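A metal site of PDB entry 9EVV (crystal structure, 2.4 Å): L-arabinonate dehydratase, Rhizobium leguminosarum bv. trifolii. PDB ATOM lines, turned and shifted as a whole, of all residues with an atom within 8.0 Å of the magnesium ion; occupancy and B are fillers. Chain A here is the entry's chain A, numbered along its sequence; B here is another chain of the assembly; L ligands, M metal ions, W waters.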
ATOM      1  N   GLU A 100     -26.792  13.954  18.488  1.00  0.00           N
ATOM      2  CA  GLU A 100     -25.905  14.791  17.693  1.00  0.00           C
ATOM      3  C   GLU A 100     -26.261  14.768  16.213  1.00  0.00           C
ATOM      4  O   GLU A 100     -25.989  15.738  15.493  1.00  0.00           O
ATOM      5  CB  GLU A 100     -24.445  14.341  17.878  1.00  0.00           C
ATOM      6  CG  GLU A 100     -23.430  15.295  17.255  1.00  0.00           C
ATOM      7  CD  GLU A 100     -22.727  16.146  18.299  1.00  0.00           C
ATOM      8  OE1 GLU A 100     -23.407  16.475  19.271  1.00  0.00           O
ATOM      9  OE2 GLU A 100     -21.520  16.502  18.128  1.00  0.00           O
ATOM     10  N   THR A 106     -27.838  22.357  16.285  1.00  0.00           N
ATOM     11  CA  THR A 106     -26.713  21.572  16.786  1.00  0.00           C
ATOM     12  C   THR A 106     -27.025  21.062  18.184  1.00  0.00           C
ATOM     13  O   THR A 106     -27.593  21.779  19.009  1.00  0.00           O
ATOM     14  CB  THR A 106     -25.421  22.391  16.777  1.00  0.00           C
ATOM     15  OG1 THR A 106     -24.353  21.644  17.380  1.00  0.00           O
ATOM     16  CG2 THR A 106     -25.574  23.711  17.533  1.00  0.00           C
ATOM     17  N   ALA A 107     -26.672  19.799  18.466  1.00  0.00           N
ATOM     18  CA  ALA A 107     -27.042  19.221  19.763  1.00  0.00           C
ATOM     19  C   ALA A 107     -26.506  20.054  20.917  1.00  0.00           C
ATOM     20  O   ALA A 107     -27.108  20.075  21.985  1.00  0.00           O
ATOM     21  CB  ALA A 107     -26.532  17.775  19.858  1.00  0.00           C
ATOM     22  N   MET A 108     -25.354  20.714  20.703  1.00  0.00           N
ATOM     23  CA  MET A 108     -24.783  21.660  21.667  1.00  0.00           C
ATOM     24  C   MET A 108     -25.804  22.643  22.231  1.00  0.00           C
ATOM     25  O   MET A 108     -25.842  22.884  23.433  1.00  0.00           O
ATOM     26  CB  MET A 108     -23.623  22.413  20.993  1.00  0.00           C
ATOM     27  CG  MET A 108     -22.545  22.981  21.928  1.00  0.00           C
ATOM     28  SD  MET A 108     -22.050  22.051  23.389  1.00  0.00           S
ATOM     29  CE  MET A 108     -22.435  23.209  24.681  1.00  0.00           C
ATOM     30  N   CYS A 136     -24.117   8.922  22.760  1.00  0.00           N
ATOM     31  CA  CYS A 136     -23.916  10.021  21.819  1.00  0.00           C
ATOM     32  C   CYS A 136     -23.318  11.235  22.511  1.00  0.00           C
ATOM     33  O   CYS A 136     -23.693  11.589  23.631  1.00  0.00           O
ATOM     34  CB  CYS A 136     -25.240  10.408  21.174  1.00  0.00           C
ATOM     35  SG  CYS A 136     -25.061  10.966  19.488  1.00  0.00           S
ATOM     36  N   ASP A 137     -22.398  11.896  21.797  1.00  0.00           N
ATOM     37  CA  ASP A 137     -21.682  13.106  22.246  1.00  0.00           C
ATOM     38  C   ASP A 137     -22.224  13.850  23.484  1.00  0.00           C
ATOM     39  O   ASP A 137     -21.629  13.832  24.562  1.00  0.00           O
ATOM     40  CB  ASP A 137     -21.611  14.100  21.079  1.00  0.00           C
ATOM     41  CG  ASP A 137     -20.801  13.544  19.908  1.00  0.00           C
ATOM     42  OD1 ASP A 137     -20.429  12.354  19.993  1.00  0.00           O
ATOM     43  OD2 ASP A 137     -20.517  14.268  18.938  1.00  0.00           O
ATOM     44  N   KCX A 138     -23.366  14.509  23.338  1.00  0.00           N
ATOM     45  CA  KCX A 138     -23.790  15.429  24.380  1.00  0.00           C
ATOM     46  CB  KCX A 138     -24.563  16.588  23.742  1.00  0.00           C
ATOM     47  CG  KCX A 138     -23.674  17.796  23.568  1.00  0.00           C
ATOM     48  CD  KCX A 138     -23.243  17.936  22.148  1.00  0.00           C
ATOM     49  CE  KCX A 138     -22.002  18.799  21.968  1.00  0.00           C
ATOM     50  NZ  KCX A 138     -21.433  18.174  20.760  1.00  0.00           N
ATOM     51  C   KCX A 138     -24.620  14.791  25.513  1.00  0.00           C
ATOM     52  O   KCX A 138     -24.957  15.460  26.500  1.00  0.00           O
ATOM     53  CX  KCX A 138     -20.230  17.611  20.824  1.00  0.00           C
ATOM     54  OQ1 KCX A 138     -19.607  17.688  21.897  1.00  0.00           O
ATOM     55  OQ2 KCX A 138     -19.742  17.050  19.827  1.00  0.00           O
ATOM     56  N   TRP A 179     -14.912  13.952   6.457  1.00  0.00           N
ATOM     57  CA  TRP A 179     -14.144  15.133   6.038  1.00  0.00           C
ATOM     58  C   TRP A 179     -13.138  14.773   4.954  1.00  0.00           C
ATOM     59  O   TRP A 179     -13.091  15.418   3.901  1.00  0.00           O
ATOM     60  CB  TRP A 179     -13.430  15.781   7.225  1.00  0.00           C
ATOM     61  CG  TRP A 179     -14.100  15.614   8.577  1.00  0.00           C
ATOM     62  CD1 TRP A 179     -13.591  14.942   9.651  1.00  0.00           C
ATOM     63  CD2 TRP A 179     -15.360  16.168   9.001  1.00  0.00           C
ATOM     64  NE1 TRP A 179     -14.470  15.018  10.706  1.00  0.00           N
ATOM     65  CE2 TRP A 179     -15.560  15.761  10.339  1.00  0.00           C
ATOM     66  CE3 TRP A 179     -16.342  16.939   8.376  1.00  0.00           C
ATOM     67  CZ2 TRP A 179     -16.709  16.103  11.069  1.00  0.00           C
ATOM     68  CZ3 TRP A 179     -17.492  17.281   9.106  1.00  0.00           C
ATOM     69  CH2 TRP A 179     -17.662  16.858  10.431  1.00  0.00           C
ATOM     70  N   CYS A 209     -19.781   6.914  17.516  1.00  0.00           N
ATOM     71  CA  CYS A 209     -18.690   7.068  16.576  1.00  0.00           C
ATOM     72  C   CYS A 209     -17.464   6.287  17.026  1.00  0.00           C
ATOM     73  O   CYS A 209     -17.098   6.315  18.210  1.00  0.00           O
ATOM     74  CB  CYS A 209     -18.340   8.537  16.425  1.00  0.00           C
ATOM     75  SG  CYS A 209     -19.682   9.451  15.696  1.00  0.00           S
ATOM     76  N   GLY A 213     -13.405  10.595  18.880  1.00  0.00           N
ATOM     77  CA  GLY A 213     -14.213  11.796  18.876  1.00  0.00           C
ATOM     78  C   GLY A 213     -14.781  12.095  20.243  1.00  0.00           C
ATOM     79  O   GLY A 213     -14.287  11.610  21.272  1.00  0.00           O
ATOM     80  N   THR A 214     -15.839  12.922  20.259  1.00  0.00           N
ATOM     81  CA  THR A 214     -16.378  13.422  21.521  1.00  0.00           C
ATOM     82  C   THR A 214     -17.012  12.301  22.334  1.00  0.00           C
ATOM     83  O   THR A 214     -16.926  12.283  23.574  1.00  0.00           O
ATOM     84  CB  THR A 214     -17.438  14.510  21.276  1.00  0.00           C
ATOM     85  OG1 THR A 214     -16.925  15.548  20.431  1.00  0.00           O
ATOM     86  CG2 THR A 214     -17.858  15.097  22.637  1.00  0.00           C
ATOM     87  N   ALA A 215     -17.695  11.373  21.655  1.00  0.00           N
ATOM     88  CA  ALA A 215     -18.363  10.317  22.377  1.00  0.00           C
ATOM     89  C   ALA A 215     -17.351   9.342  22.964  1.00  0.00           C
ATOM     90  O   ALA A 215     -17.503   8.904  24.119  1.00  0.00           O
ATOM     91  CB  ALA A 215     -19.361   9.607  21.474  1.00  0.00           C
ATOM     92  N   SER A 285     -11.086  14.731  21.958  1.00  0.00           N
ATOM     93  CA  SER A 285     -11.810  15.839  21.340  1.00  0.00           C
ATOM     94  C   SER A 285     -11.583  17.146  22.092  1.00  0.00           C
ATOM     95  O   SER A 285     -11.447  17.179  23.315  1.00  0.00           O
ATOM     96  CB  SER A 285     -13.309  15.525  21.308  1.00  0.00           C
ATOM     97  OG  SER A 285     -14.085  16.686  20.996  1.00  0.00           O
ATOM     98  N   ASN A 287     -13.941  19.428  22.279  1.00  0.00           N
ATOM     99  CA  ASN A 287     -15.161  19.623  23.049  1.00  0.00           C
ATOM    100  C   ASN A 287     -15.004  19.135  24.474  1.00  0.00           C
ATOM    101  O   ASN A 287     -15.702  19.599  25.376  1.00  0.00           O
ATOM    102  CB  ASN A 287     -16.347  18.909  22.384  1.00  0.00           C
ATOM    103  CG  ASN A 287     -16.607  19.422  20.981  1.00  0.00           C
ATOM    104  OD1 ASN A 287     -16.403  20.611  20.684  1.00  0.00           O
ATOM    105  ND2 ASN A 287     -17.038  18.527  20.116  1.00  0.00           N
ATOM    106  N   HIS A 291     -17.150  20.713  27.757  1.00  0.00           N
ATOM    107  CA  HIS A 291     -17.970  19.835  28.609  1.00  0.00           C
ATOM    108  C   HIS A 291     -17.366  19.682  29.997  1.00  0.00           C
ATOM    109  O   HIS A 291     -18.088  19.641  31.001  1.00  0.00           O
ATOM    110  CB  HIS A 291     -18.163  18.477  27.937  1.00  0.00           C
ATOM    111  CG  HIS A 291     -18.901  18.542  26.640  1.00  0.00           C
ATOM    112  ND1 HIS A 291     -19.963  19.403  26.433  1.00  0.00           N
ATOM    113  CD2 HIS A 291     -18.717  17.896  25.468  1.00  0.00           C
ATOM    114  CE1 HIS A 291     -20.401  19.276  25.195  1.00  0.00           C
ATOM    115  NE2 HIS A 291     -19.657  18.368  24.587  1.00  0.00           N
ATOM    116  N   GLU A 462     -20.335  22.746  15.181  1.00  0.00           N
ATOM    117  CA  GLU A 462     -19.033  22.177  14.848  1.00  0.00           C
ATOM    118  C   GLU A 462     -18.715  22.542  13.404  1.00  0.00           C
ATOM    119  O   GLU A 462     -18.863  21.750  12.485  1.00  0.00           O
ATOM    120  CB  GLU A 462     -19.045  20.665  15.032  1.00  0.00           C
ATOM    121  CG  GLU A 462     -19.287  20.187  16.436  1.00  0.00           C
ATOM    122  CD  GLU A 462     -19.413  18.680  16.482  1.00  0.00           C
ATOM    123  OE1 GLU A 462     -19.448  18.068  15.391  1.00  0.00           O
ATOM    124  OE2 GLU A 462     -19.498  18.103  17.599  1.00  0.00           O
ATOM    125  N   ARG A 487     -16.958  25.358  17.445  1.00  0.00           N
ATOM    126  CA  ARG A 487     -16.270  24.138  17.821  1.00  0.00           C
ATOM    127  C   ARG A 487     -15.890  23.368  16.560  1.00  0.00           C
ATOM    128  O   ARG A 487     -16.087  23.839  15.430  1.00  0.00           O
ATOM    129  CB  ARG A 487     -17.148  23.273  18.730  1.00  0.00           C
ATOM    130  CG  ARG A 487     -17.543  23.881  20.061  1.00  0.00           C
ATOM    131  CD  ARG A 487     -18.574  22.980  20.791  1.00  0.00           C
ATOM    132  NE  ARG A 487     -19.844  22.880  20.066  1.00  0.00           N
ATOM    133  CZ  ARG A 487     -20.311  21.760  19.512  1.00  0.00           C
ATOM    134  NH1 ARG A 487     -19.669  20.598  19.586  1.00  0.00           N
ATOM    135  NH2 ARG A 487     -21.467  21.813  18.839  1.00  0.00           N
ATOM    136  N   MET A 488     -15.367  22.167  16.744  1.00  0.00           N
ATOM    137  CA  MET A 488     -15.209  21.256  15.616  1.00  0.00           C
ATOM    138  C   MET A 488     -15.535  19.871  16.132  1.00  0.00           C
ATOM    139  O   MET A 488     -15.545  19.637  17.331  1.00  0.00           O
ATOM    140  CB  MET A 488     -13.806  21.354  15.011  1.00  0.00           C
ATOM    141  CG  MET A 488     -12.752  20.423  15.552  1.00  0.00           C
ATOM    142  SD  MET A 488     -11.208  20.795  14.638  1.00  0.00           S
ATOM    143  CE  MET A 488     -10.032  19.678  15.451  1.00  0.00           C
ATOM    144  N   SER A 489     -15.871  18.952  15.226  1.00  0.00           N
ATOM    145  CA  SER A 489     -16.130  17.605  15.718  1.00  0.00           C
ATOM    146  C   SER A 489     -14.902  17.051  16.433  1.00  0.00           C
ATOM    147  O   SER A 489     -13.763  17.383  16.103  1.00  0.00           O
ATOM    148  CB  SER A 489     -16.520  16.662  14.594  1.00  0.00           C
ATOM    149  OG  SER A 489     -16.502  15.350  15.105  1.00  0.00           O
ATOM    150  N   GLY A 490     -15.150  16.191  17.421  1.00  0.00           N
ATOM    151  CA  GLY A 490     -14.056  15.419  17.990  1.00  0.00           C
ATOM    152  C   GLY A 490     -13.309  14.601  16.966  1.00  0.00           C
ATOM    153  O   GLY A 490     -12.133  14.254  17.198  1.00  0.00           O
ATOM    154  N   THR A 491     -13.935  14.314  15.824  1.00  0.00           N
ATOM    155  CA  THR A 491     -13.321  13.534  14.760  1.00  0.00           C
ATOM    156  C   THR A 491     -12.533  14.370  13.755  1.00  0.00           C
ATOM    157  O   THR A 491     -11.865  13.791  12.889  1.00  0.00           O
ATOM    158  CB  THR A 491     -14.389  12.771  13.978  1.00  0.00           C
ATOM    159  OG1 THR A 491     -15.268  13.710  13.335  1.00  0.00           O
ATOM    160  CG2 THR A 491     -15.183  11.860  14.914  1.00  0.00           C
ATOM    161  N   TYR B  35     -24.413  11.881   6.266  1.00  0.00           N
ATOM    162  CA  TYR B  35     -24.194  11.773   7.695  1.00  0.00           C
ATOM    163  C   TYR B  35     -25.495  11.421   8.413  1.00  0.00           C
ATOM    164  O   TYR B  35     -25.585  10.387   9.098  1.00  0.00           O
ATOM    165  CB  TYR B  35     -23.591  13.080   8.218  1.00  0.00           C
ATOM    166  CG  TYR B  35     -23.648  13.312   9.720  1.00  0.00           C
ATOM    167  CD1 TYR B  35     -23.137  12.363  10.599  1.00  0.00           C
ATOM    168  CD2 TYR B  35     -24.202  14.477  10.259  1.00  0.00           C
ATOM    169  CE1 TYR B  35     -23.178  12.555  11.982  1.00  0.00           C
ATOM    170  CE2 TYR B  35     -24.243  14.683  11.632  1.00  0.00           C
ATOM    171  CZ  TYR B  35     -23.731  13.717  12.488  1.00  0.00           C
ATOM    172  OH  TYR B  35     -23.759  13.874  13.853  1.00  0.00           O
HETATM  173 FE1  LIG L   1     -23.569  10.036  17.947  1.00  0.00          FE
HETATM  174 FE2  LIG L   1     -21.240  10.876  16.804  1.00  0.00          FE
HETATM  175  S1  LIG L   1     -23.305  11.188  16.065  1.00  0.00           S
HETATM  176  S2  LIG L   1     -21.487   9.725  18.668  1.00  0.00           S
HETATM  177 MG    MG M   1     -19.402  16.059  18.175  1.00  0.00          MG
HETATM  178  O   HOH W   1     -19.740  15.450  16.190  1.00  0.00           O
HETATM  179  O   HOH W   2     -17.584  14.896  17.826  1.00  0.00           O
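A sulfur (S1) of the ligand sits close to the side-chain hydroxyl of Tyr 35 of chain B, at 3.5 Å.
A sulfur (S2) of the ligand lies close to the backbone NH (N) of Cys 209.
FE2 of the ligand is bound by SG of Cys 209, at 2.4 Å.
The side-chain sulfur (SG) of Cys 136 is bound to an iron atom (FE1) of the ligand, at 2.3 Å.
OQ2 of KCX 138 sits close to the side-chain hydroxyl (OG1) of Thr 214, 3.2 Å away.
The guanidinium group of Arg 487 lies within salt-bridge range of OQ1 of KCX 138.
NE2 of His 291 sits at hydrogen-bond distance from OQ1 of KCX 138 (2.8 Å).
OE2 of Glu 462 sits close to NH1 of Arg 487 (3.2 Å).
The backbone NH of Ala 215 lies close to the side-chain carboxylate of Asp 137 (3.3 Å).
The side-chain hydroxyl (OG1) of Thr 214 lies within hydrogen-bond range of the side-chain hydroxyl (OG) of Ser 285, at 3.1 Å.
The side-chain amide nitrogen (ND2) of Asn 287 lies close to the guanidinium group (NH1) of Arg 487 (3.4 Å).
The side-chain amide nitrogen (ND2) of Asn 287 is in hydrogen-bond range of the backbone carbonyl oxygen (O) of Met 488 (3.3 Å).
Thr 214 touches the magnesium ion (OG1 to MG, 3.4 Å).
Asn 287 touches the magnesium ion (ND2 to MG, 3.9 Å).
Of the 22 residues printed, 6 come within 4 Å of the magnesium ion.
The magnesium ion is bound by OQ2 of KCX 138, 2.0 Å away.
Water W1 is bound to the magnesium ion (2.1 Å).
The magnesium ion is bound by OE2 of Glu 462 (2.1 Å).
The magnesium ion is bound by OE2 of Glu 100 (2.2 Å).
Water W2 binds the magnesium ion, at 2.2 Å.
The magnesium ion is bound by OD2 of Asp 137 (2.2 Å).
The magnesium ion has six donor atoms within binding distance.
Water W2 lies within hydrogen-bond range of OG1 of Thr 214 (2.8 Å), N of Gly 490 (2.8 Å) and OG of Ser 489 (3.0 Å).
Water W1 lies within hydrogen-bond range of the side-chain carboxylate of Glu 462 (2.8 Å) and the side-chain hydroxyl of Ser 489 (3.4 Å).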
